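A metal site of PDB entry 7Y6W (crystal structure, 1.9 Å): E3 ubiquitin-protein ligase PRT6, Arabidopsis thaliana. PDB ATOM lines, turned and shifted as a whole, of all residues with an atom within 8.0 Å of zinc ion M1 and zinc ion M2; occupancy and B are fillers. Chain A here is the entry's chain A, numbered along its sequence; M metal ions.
The side-chain sulfur of Cys 72 sits close to the backbone NH of Asn 74, at 3.5 Å.
N of Cys 9 lies within hydrogen-bond range of O of Cys 60, 3.0 Å away.
The side-chain sulfur (SG) of Cys 58 sits close to the backbone NH (N) of Cys 60 (3.5 Å).
The backbone carbonyl oxygen (O) of Ser 11 sits at hydrogen-bond distance from the backbone NH (N) of Cys 58, at 2.9 Å.
The side-chain sulfur (SG) of Cys 9 sits close to the backbone NH (N) of Ser 11 (3.6 Å).
Within 4 Å of zinc ion M1: Cys 9, Cys 34, Cys 37 and Cys 58.
The nearest printed residue that does not touch zinc ion M1 is Cys 60 (4.2 Å).
Zinc ion M1 is bound by SG of Cys 9 (2.2 Å), SG of Cys 58 (2.3 Å), SG of Cys 37 (2.3 Å) and SG of Cys 34 (2.3 Å).
Zinc ion M1 has four donor atoms within binding distance.
Zinc ion M2 is bound by ND1 of His 75, SG of Cys 72, SG of Cys 60 and SG of Cys 37.
Zinc ion M2 has four donor atoms within binding distance.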
ATOM      1  N   GLY A   7      -9.325  -1.830 -13.357  1.00  0.00           N
ATOM      2  CA  GLY A   7     -10.401  -1.152 -12.641  1.00  0.00           C
ATOM      3  C   GLY A   7     -11.394  -0.437 -13.543  1.00  0.00           C
ATOM      4  O   GLY A   7     -11.002   0.226 -14.510  1.00  0.00           O
ATOM      5  N   VAL A   8     -12.692  -0.597 -13.249  1.00  0.00           N
ATOM      6  CA  VAL A   8     -13.747   0.224 -13.839  1.00  0.00           C
ATOM      7  C   VAL A   8     -14.161   1.219 -12.755  1.00  0.00           C
ATOM      8  O   VAL A   8     -14.122   0.914 -11.572  1.00  0.00           O
ATOM      9  CB  VAL A   8     -14.968  -0.594 -14.326  1.00  0.00           C
ATOM     10  CG1 VAL A   8     -16.102   0.338 -14.709  1.00  0.00           C
ATOM     11  CG2 VAL A   8     -14.584  -1.472 -15.498  1.00  0.00           C
ATOM     12  N   CYS A   9     -14.564   2.425 -13.177  1.00  0.00           N
ATOM     13  CA  CYS A   9     -14.924   3.456 -12.212  1.00  0.00           C
ATOM     14  C   CYS A   9     -16.193   3.069 -11.451  1.00  0.00           C
ATOM     15  O   CYS A   9     -16.228   3.080 -10.222  1.00  0.00           O
ATOM     16  CB  CYS A   9     -15.132   4.802 -12.891  1.00  0.00           C
ATOM     17  SG  CYS A   9     -15.739   6.067 -11.721  1.00  0.00           S
ATOM     18  N   GLY A  10     -17.253   2.783 -12.187  1.00  0.00           N
ATOM     19  CA  GLY A  10     -18.506   2.322 -11.619  1.00  0.00           C
ATOM     20  C   GLY A  10     -19.254   3.308 -10.740  1.00  0.00           C
ATOM     21  O   GLY A  10     -20.304   2.928 -10.214  1.00  0.00           O
ATOM     22  N   SER A  11     -18.756   4.536 -10.571  1.00  0.00           N
ATOM     23  CA  SER A  11     -19.437   5.515  -9.727  1.00  0.00           C
ATOM     24  C   SER A  11     -20.884   5.711 -10.160  1.00  0.00           C
ATOM     25  O   SER A  11     -21.171   5.761 -11.358  1.00  0.00           O
ATOM     26  CB  SER A  11     -18.705   6.854  -9.777  1.00  0.00           C
ATOM     27  OG  SER A  11     -19.616   7.930  -9.672  1.00  0.00           O
ATOM     28  N   VAL A  12     -21.780   5.881  -9.200  1.00  0.00           N
ATOM     29  CA  VAL A  12     -23.206   5.822  -9.483  1.00  0.00           C
ATOM     30  C   VAL A  12     -23.839   7.197  -9.378  1.00  0.00           C
ATOM     31  O   VAL A  12     -23.562   7.968  -8.452  1.00  0.00           O
ATOM     32  CB  VAL A  12     -23.928   4.826  -8.562  1.00  0.00           C
ATOM     33  CG1 VAL A  12     -25.442   4.887  -8.783  1.00  0.00           C
ATOM     34  CG2 VAL A  12     -23.439   3.424  -8.818  1.00  0.00           C
ATOM     35  N   TRP A  13     -24.746   7.484 -10.305  1.00  0.00           N
ATOM     36  CA  TRP A  13     -25.461   8.749 -10.344  1.00  0.00           C
ATOM     37  C   TRP A  13     -26.891   8.550  -9.880  1.00  0.00           C
ATOM     38  O   TRP A  13     -27.513   7.523 -10.165  1.00  0.00           O
ATOM     39  CB  TRP A  13     -25.484   9.359 -11.745  1.00  0.00           C
ATOM     40  CG  TRP A  13     -24.143   9.606 -12.268  1.00  0.00           C
ATOM     41  CD1 TRP A  13     -23.166  10.322 -11.670  1.00  0.00           C
ATOM     42  CD2 TRP A  13     -23.613   9.111 -13.485  1.00  0.00           C
ATOM     43  NE1 TRP A  13     -22.048  10.321 -12.458  1.00  0.00           N
ATOM     44  CE2 TRP A  13     -22.292   9.573 -13.570  1.00  0.00           C
ATOM     45  CE3 TRP A  13     -24.132   8.337 -14.532  1.00  0.00           C
ATOM     46  CZ2 TRP A  13     -21.471   9.275 -14.648  1.00  0.00           C
ATOM     47  CZ3 TRP A  13     -23.326   8.046 -15.605  1.00  0.00           C
ATOM     48  CH2 TRP A  13     -21.998   8.512 -15.655  1.00  0.00           C
ATOM     49  N   ALA A  32     -21.582   7.460 -20.611  1.00  0.00           N
ATOM     50  CA  ALA A  32     -21.232   8.715 -19.961  1.00  0.00           C
ATOM     51  C   ALA A  32     -20.139   8.434 -18.948  1.00  0.00           C
ATOM     52  O   ALA A  32     -19.948   7.287 -18.526  1.00  0.00           O
ATOM     53  CB  ALA A  32     -22.437   9.357 -19.276  1.00  0.00           C
ATOM     54  N   ILE A  33     -19.408   9.480 -18.562  1.00  0.00           N
ATOM     55  CA  ILE A  33     -18.413   9.332 -17.499  1.00  0.00           C
ATOM     56  C   ILE A  33     -18.573  10.425 -16.448  1.00  0.00           C
ATOM     57  O   ILE A  33     -19.031  11.531 -16.756  1.00  0.00           O
ATOM     58  CB  ILE A  33     -16.977   9.335 -18.056  1.00  0.00           C
ATOM     59  CG1 ILE A  33     -16.707  10.585 -18.881  1.00  0.00           C
ATOM     60  CG2 ILE A  33     -16.733   8.112 -18.938  1.00  0.00           C
ATOM     61  CD1 ILE A  33     -15.257  10.769 -19.219  1.00  0.00           C
ATOM     62  N   CYS A  34     -18.170  10.122 -15.225  1.00  0.00           N
ATOM     63  CA  CYS A  34     -18.335  11.075 -14.136  1.00  0.00           C
ATOM     64  C   CYS A  34     -17.392  12.252 -14.323  1.00  0.00           C
ATOM     65  O   CYS A  34     -16.400  12.201 -15.069  1.00  0.00           O
ATOM     66  CB  CYS A  34     -18.130  10.381 -12.772  1.00  0.00           C
ATOM     67  SG  CYS A  34     -16.489   9.850 -12.465  1.00  0.00           S
ATOM     68  N   VAL A  35     -17.750  13.376 -13.685  1.00  0.00           N
ATOM     69  CA  VAL A  35     -16.956  14.599 -13.840  1.00  0.00           C
ATOM     70  C   VAL A  35     -15.502  14.339 -13.471  1.00  0.00           C
ATOM     71  O   VAL A  35     -14.610  14.846 -14.188  1.00  0.00           O
ATOM     72  CB  VAL A  35     -17.574  15.751 -13.050  1.00  0.00           C
ATOM     73  CG1 VAL A  35     -16.586  16.942 -12.991  1.00  0.00           C
ATOM     74  CG2 VAL A  35     -18.877  16.160 -13.640  1.00  0.00           C
ATOM     75  N   PRO A  36     -15.186  13.677 -12.374  1.00  0.00           N
ATOM     76  CA  PRO A  36     -13.769  13.440 -12.053  1.00  0.00           C
ATOM     77  C   PRO A  36     -13.031  12.652 -13.125  1.00  0.00           C
ATOM     78  O   PRO A  36     -11.867  12.956 -13.431  1.00  0.00           O
ATOM     79  CB  PRO A  36     -13.814  12.643 -10.738  1.00  0.00           C
ATOM     80  CG  PRO A  36     -15.187  12.807 -10.205  1.00  0.00           C
ATOM     81  CD  PRO A  36     -16.091  13.109 -11.354  1.00  0.00           C
ATOM     82  N   CYS A  37     -13.659  11.631 -13.687  1.00  0.00           N
ATOM     83  CA  CYS A  37     -12.981  10.872 -14.740  1.00  0.00           C
ATOM     84  C   CYS A  37     -12.800  11.734 -15.981  1.00  0.00           C
ATOM     85  O   CYS A  37     -11.779  11.655 -16.678  1.00  0.00           O
ATOM     86  CB  CYS A  37     -13.797   9.608 -15.068  1.00  0.00           C
ATOM     87  SG  CYS A  37     -13.823   8.249 -13.693  1.00  0.00           S
ATOM     88  N   PHE A  38     -13.772  12.587 -16.283  1.00  0.00           N
ATOM     89  CA  PHE A  38     -13.614  13.478 -17.412  1.00  0.00           C
ATOM     90  C   PHE A  38     -12.422  14.398 -17.177  1.00  0.00           C
ATOM     91  O   PHE A  38     -11.571  14.546 -18.063  1.00  0.00           O
ATOM     92  CB  PHE A  38     -14.903  14.287 -17.668  1.00  0.00           C
ATOM     93  CG  PHE A  38     -14.811  15.222 -18.863  1.00  0.00           C
ATOM     94  CD1 PHE A  38     -15.127  14.800 -20.121  1.00  0.00           C
ATOM     95  CD2 PHE A  38     -14.348  16.508 -18.703  1.00  0.00           C
ATOM     96  CE1 PHE A  38     -15.015  15.626 -21.211  1.00  0.00           C
ATOM     97  CE2 PHE A  38     -14.245  17.358 -19.774  1.00  0.00           C
ATOM     98  CZ  PHE A  38     -14.584  16.915 -21.033  1.00  0.00           C
ATOM     99  N   ASN A  40      -9.780  14.076 -15.406  1.00  0.00           N
ATOM    100  CA  ASN A  40      -8.507  13.378 -15.332  1.00  0.00           C
ATOM    101  C   ASN A  40      -8.196  12.597 -16.610  1.00  0.00           C
ATOM    102  O   ASN A  40      -7.248  11.805 -16.629  1.00  0.00           O
ATOM    103  CB  ASN A  40      -8.510  12.443 -14.110  1.00  0.00           C
ATOM    104  CG  ASN A  40      -8.521  13.206 -12.812  1.00  0.00           C
ATOM    105  OD1 ASN A  40      -7.831  14.209 -12.674  1.00  0.00           O
ATOM    106  ND2 ASN A  40      -9.304  12.746 -11.851  1.00  0.00           N
ATOM    107  N   GLY A  41      -8.968  12.835 -17.668  1.00  0.00           N
ATOM    108  CA  GLY A  41      -8.660  12.346 -18.996  1.00  0.00           C
ATOM    109  C   GLY A  41      -8.308  13.473 -19.955  1.00  0.00           C
ATOM    110  O   GLY A  41      -8.116  14.630 -19.582  1.00  0.00           O
ATOM    111  N   CYS A  57     -24.349   4.717 -14.224  1.00  0.00           N
ATOM    112  CA  CYS A  57     -23.012   4.584 -13.667  1.00  0.00           C
ATOM    113  C   CYS A  57     -21.966   4.939 -14.710  1.00  0.00           C
ATOM    114  O   CYS A  57     -22.167   4.775 -15.914  1.00  0.00           O
ATOM    115  CB  CYS A  57     -22.778   3.169 -13.132  1.00  0.00           C
ATOM    116  SG  CYS A  57     -22.839   1.868 -14.438  1.00  0.00           S
ATOM    117  N   CYS A  58     -20.822   5.417 -14.226  1.00  0.00           N
ATOM    118  CA  CYS A  58     -19.741   5.880 -15.081  1.00  0.00           C
ATOM    119  C   CYS A  58     -19.111   4.733 -15.860  1.00  0.00           C
ATOM    120  O   CYS A  58     -18.874   3.642 -15.324  1.00  0.00           O
ATOM    121  CB  CYS A  58     -18.685   6.595 -14.234  1.00  0.00           C
ATOM    122  SG  CYS A  58     -17.187   7.083 -14.983  1.00  0.00           S
ATOM    123  N   ASP A  59     -18.820   4.977 -17.137  1.00  0.00           N
ATOM    124  CA  ASP A  59     -18.273   3.969 -18.017  1.00  0.00           C
ATOM    125  C   ASP A  59     -16.743   4.006 -18.149  1.00  0.00           C
ATOM    126  O   ASP A  59     -16.185   3.192 -18.882  1.00  0.00           O
ATOM    127  CB  ASP A  59     -18.912   4.111 -19.407  1.00  0.00           C
ATOM    128  CG  ASP A  59     -20.416   3.834 -19.384  1.00  0.00           C
ATOM    129  OD1 ASP A  59     -20.841   2.765 -18.886  1.00  0.00           O
ATOM    130  OD2 ASP A  59     -21.192   4.696 -19.862  1.00  0.00           O
ATOM    131  N   CYS A  60     -16.071   4.926 -17.458  1.00  0.00           N
ATOM    132  CA  CYS A  60     -14.620   5.023 -17.534  1.00  0.00           C
ATOM    133  C   CYS A  60     -13.995   3.708 -17.087  1.00  0.00           C
ATOM    134  O   CYS A  60     -14.333   3.177 -16.034  1.00  0.00           O
ATOM    135  CB  CYS A  60     -14.115   6.169 -16.670  1.00  0.00           C
ATOM    136  SG  CYS A  60     -12.376   6.432 -16.860  1.00  0.00           S
ATOM    137  N   GLY A  61     -13.060   3.194 -17.893  1.00  0.00           N
ATOM    138  CA  GLY A  61     -12.421   1.927 -17.603  1.00  0.00           C
ATOM    139  C   GLY A  61     -13.028   0.744 -18.306  1.00  0.00           C
ATOM    140  O   GLY A  61     -12.376  -0.297 -18.414  1.00  0.00           O
ATOM    141  N   ASP A  62     -14.254   0.875 -18.808  1.00  0.00           N
ATOM    142  CA  ASP A  62     -15.005  -0.218 -19.411  1.00  0.00           C
ATOM    143  C   ASP A  62     -14.902  -0.104 -20.920  1.00  0.00           C
ATOM    144  O   ASP A  62     -15.612   0.683 -21.532  1.00  0.00           O
ATOM    145  CB  ASP A  62     -16.454  -0.165 -18.958  1.00  0.00           C
ATOM    146  CG  ASP A  62     -17.303  -1.263 -19.585  1.00  0.00           C
ATOM    147  OD1 ASP A  62     -16.766  -2.103 -20.364  1.00  0.00           O
ATOM    148  OD2 ASP A  62     -18.511  -1.317 -19.305  1.00  0.00           O
ATOM    149  N   TRP A  66     -16.730   2.522 -23.636  1.00  0.00           N
ATOM    150  CA  TRP A  66     -15.998   3.781 -23.727  1.00  0.00           C
ATOM    151  C   TRP A  66     -14.685   3.452 -24.398  1.00  0.00           C
ATOM    152  O   TRP A  66     -14.073   2.432 -24.080  1.00  0.00           O
ATOM    153  CB  TRP A  66     -15.781   4.375 -22.335  1.00  0.00           C
ATOM    154  CG  TRP A  66     -15.503   5.824 -22.295  1.00  0.00           C
ATOM    155  CD1 TRP A  66     -14.275   6.410 -22.199  1.00  0.00           C
ATOM    156  CD2 TRP A  66     -16.458   6.886 -22.348  1.00  0.00           C
ATOM    157  NE1 TRP A  66     -14.419   7.770 -22.158  1.00  0.00           N
ATOM    158  CE2 TRP A  66     -15.739   8.091 -22.290  1.00  0.00           C
ATOM    159  CE3 TRP A  66     -17.850   6.936 -22.444  1.00  0.00           C
ATOM    160  CZ2 TRP A  66     -16.355   9.327 -22.293  1.00  0.00           C
ATOM    161  CZ3 TRP A  66     -18.457   8.148 -22.465  1.00  0.00           C
ATOM    162  CH2 TRP A  66     -17.719   9.338 -22.369  1.00  0.00           C
ATOM    163  N   GLY A  70     -10.087   7.328 -24.097  1.00  0.00           N
ATOM    164  CA  GLY A  70     -10.891   8.240 -23.324  1.00  0.00           C
ATOM    165  C   GLY A  70     -10.895   7.981 -21.845  1.00  0.00           C
ATOM    166  O   GLY A  70     -11.546   8.713 -21.104  1.00  0.00           O
ATOM    167  N   PHE A  71     -10.160   6.973 -21.392  1.00  0.00           N
ATOM    168  CA  PHE A  71     -10.120   6.652 -19.974  1.00  0.00           C
ATOM    169  C   PHE A  71      -9.309   7.688 -19.221  1.00  0.00           C
ATOM    170  O   PHE A  71      -8.403   8.317 -19.751  1.00  0.00           O
ATOM    171  CB  PHE A  71      -9.508   5.279 -19.748  1.00  0.00           C
ATOM    172  CG  PHE A  71     -10.338   4.142 -20.257  1.00  0.00           C
ATOM    173  CD1 PHE A  71      -9.803   2.852 -20.277  1.00  0.00           C
ATOM    174  CD2 PHE A  71     -11.621   4.343 -20.731  1.00  0.00           C
ATOM    175  CE1 PHE A  71     -10.543   1.797 -20.756  1.00  0.00           C
ATOM    176  CE2 PHE A  71     -12.377   3.295 -21.168  1.00  0.00           C
ATOM    177  CZ  PHE A  71     -11.855   2.030 -21.183  1.00  0.00           C
ATOM    178  N   CYS A  72      -9.620   7.835 -17.933  1.00  0.00           N
ATOM    179  CA  CYS A  72      -8.869   8.719 -17.067  1.00  0.00           C
ATOM    180  C   CYS A  72      -7.627   7.999 -16.534  1.00  0.00           C
ATOM    181  O   CYS A  72      -7.446   6.794 -16.718  1.00  0.00           O
ATOM    182  CB  CYS A  72      -9.759   9.193 -15.915  1.00  0.00           C
ATOM    183  SG  CYS A  72      -9.956   8.056 -14.477  1.00  0.00           S
ATOM    184  N   SER A  73      -6.748   8.784 -15.889  1.00  0.00           N
ATOM    185  CA  SER A  73      -5.464   8.309 -15.378  1.00  0.00           C
ATOM    186  C   SER A  73      -5.580   7.188 -14.362  1.00  0.00           C
ATOM    187  O   SER A  73      -4.609   6.442 -14.150  1.00  0.00           O
ATOM    188  CB  SER A  73      -4.721   9.477 -14.731  1.00  0.00           C
ATOM    189  OG  SER A  73      -5.390   9.884 -13.559  1.00  0.00           O
ATOM    190  N   ASN A  74      -6.737   7.046 -13.725  1.00  0.00           N
ATOM    191  CA  ASN A  74      -6.935   6.096 -12.646  1.00  0.00           C
ATOM    192  C   ASN A  74      -7.626   4.813 -13.079  1.00  0.00           C
ATOM    193  O   ASN A  74      -7.683   3.881 -12.277  1.00  0.00           O
ATOM    194  CB  ASN A  74      -7.733   6.751 -11.512  1.00  0.00           C
ATOM    195  CG  ASN A  74      -7.032   7.972 -10.909  1.00  0.00           C
ATOM    196  OD1 ASN A  74      -5.873   7.903 -10.524  1.00  0.00           O
ATOM    197  ND2 ASN A  74      -7.752   9.091 -10.843  1.00  0.00           N
ATOM    198  N   HIS A  75      -8.091   4.699 -14.321  1.00  0.00           N
ATOM    199  CA  HIS A  75      -8.847   3.517 -14.736  1.00  0.00           C
ATOM    200  C   HIS A  75      -8.260   2.889 -15.984  1.00  0.00           C
ATOM    201  O   HIS A  75      -8.973   2.366 -16.856  1.00  0.00           O
ATOM    202  CB  HIS A  75     -10.329   3.869 -14.877  1.00  0.00           C
ATOM    203  CG  HIS A  75     -10.949   4.379 -13.611  1.00  0.00           C
ATOM    204  ND1 HIS A  75     -11.345   5.684 -13.432  1.00  0.00           N
ATOM    205  CD2 HIS A  75     -11.185   3.751 -12.423  1.00  0.00           C
ATOM    206  CE1 HIS A  75     -11.821   5.840 -12.212  1.00  0.00           C
ATOM    207  NE2 HIS A  75     -11.742   4.679 -11.574  1.00  0.00           N
ATOM    208  N   LYS A  76      -6.940   2.891 -16.086  1.00  0.00           N
ATOM    209  CA  LYS A  76      -6.267   2.174 -17.157  1.00  0.00           C
ATOM    210  C   LYS A  76      -5.478   0.984 -16.626  1.00  0.00           C
ATOM    211  O   LYS A  76      -4.834   0.283 -17.415  1.00  0.00           O
ATOM    212  CB  LYS A  76      -5.335   3.095 -17.893  1.00  0.00           C
ATOM    213  CG  LYS A  76      -5.882   4.444 -18.191  1.00  0.00           C
ATOM    214  CD  LYS A  76      -4.847   5.225 -18.936  1.00  0.00           C
ATOM    215  CE  LYS A  76      -5.508   6.226 -19.795  1.00  0.00           C
ATOM    216  NZ  LYS A  76      -4.589   7.294 -20.216  1.00  0.00           N
HETATM  217 ZN    ZN M   1     -15.965   7.732 -13.205  1.00  0.00          ZN
HETATM  218 ZN    ZN M   2     -11.904   7.064 -14.736  1.00  0.00          ZN
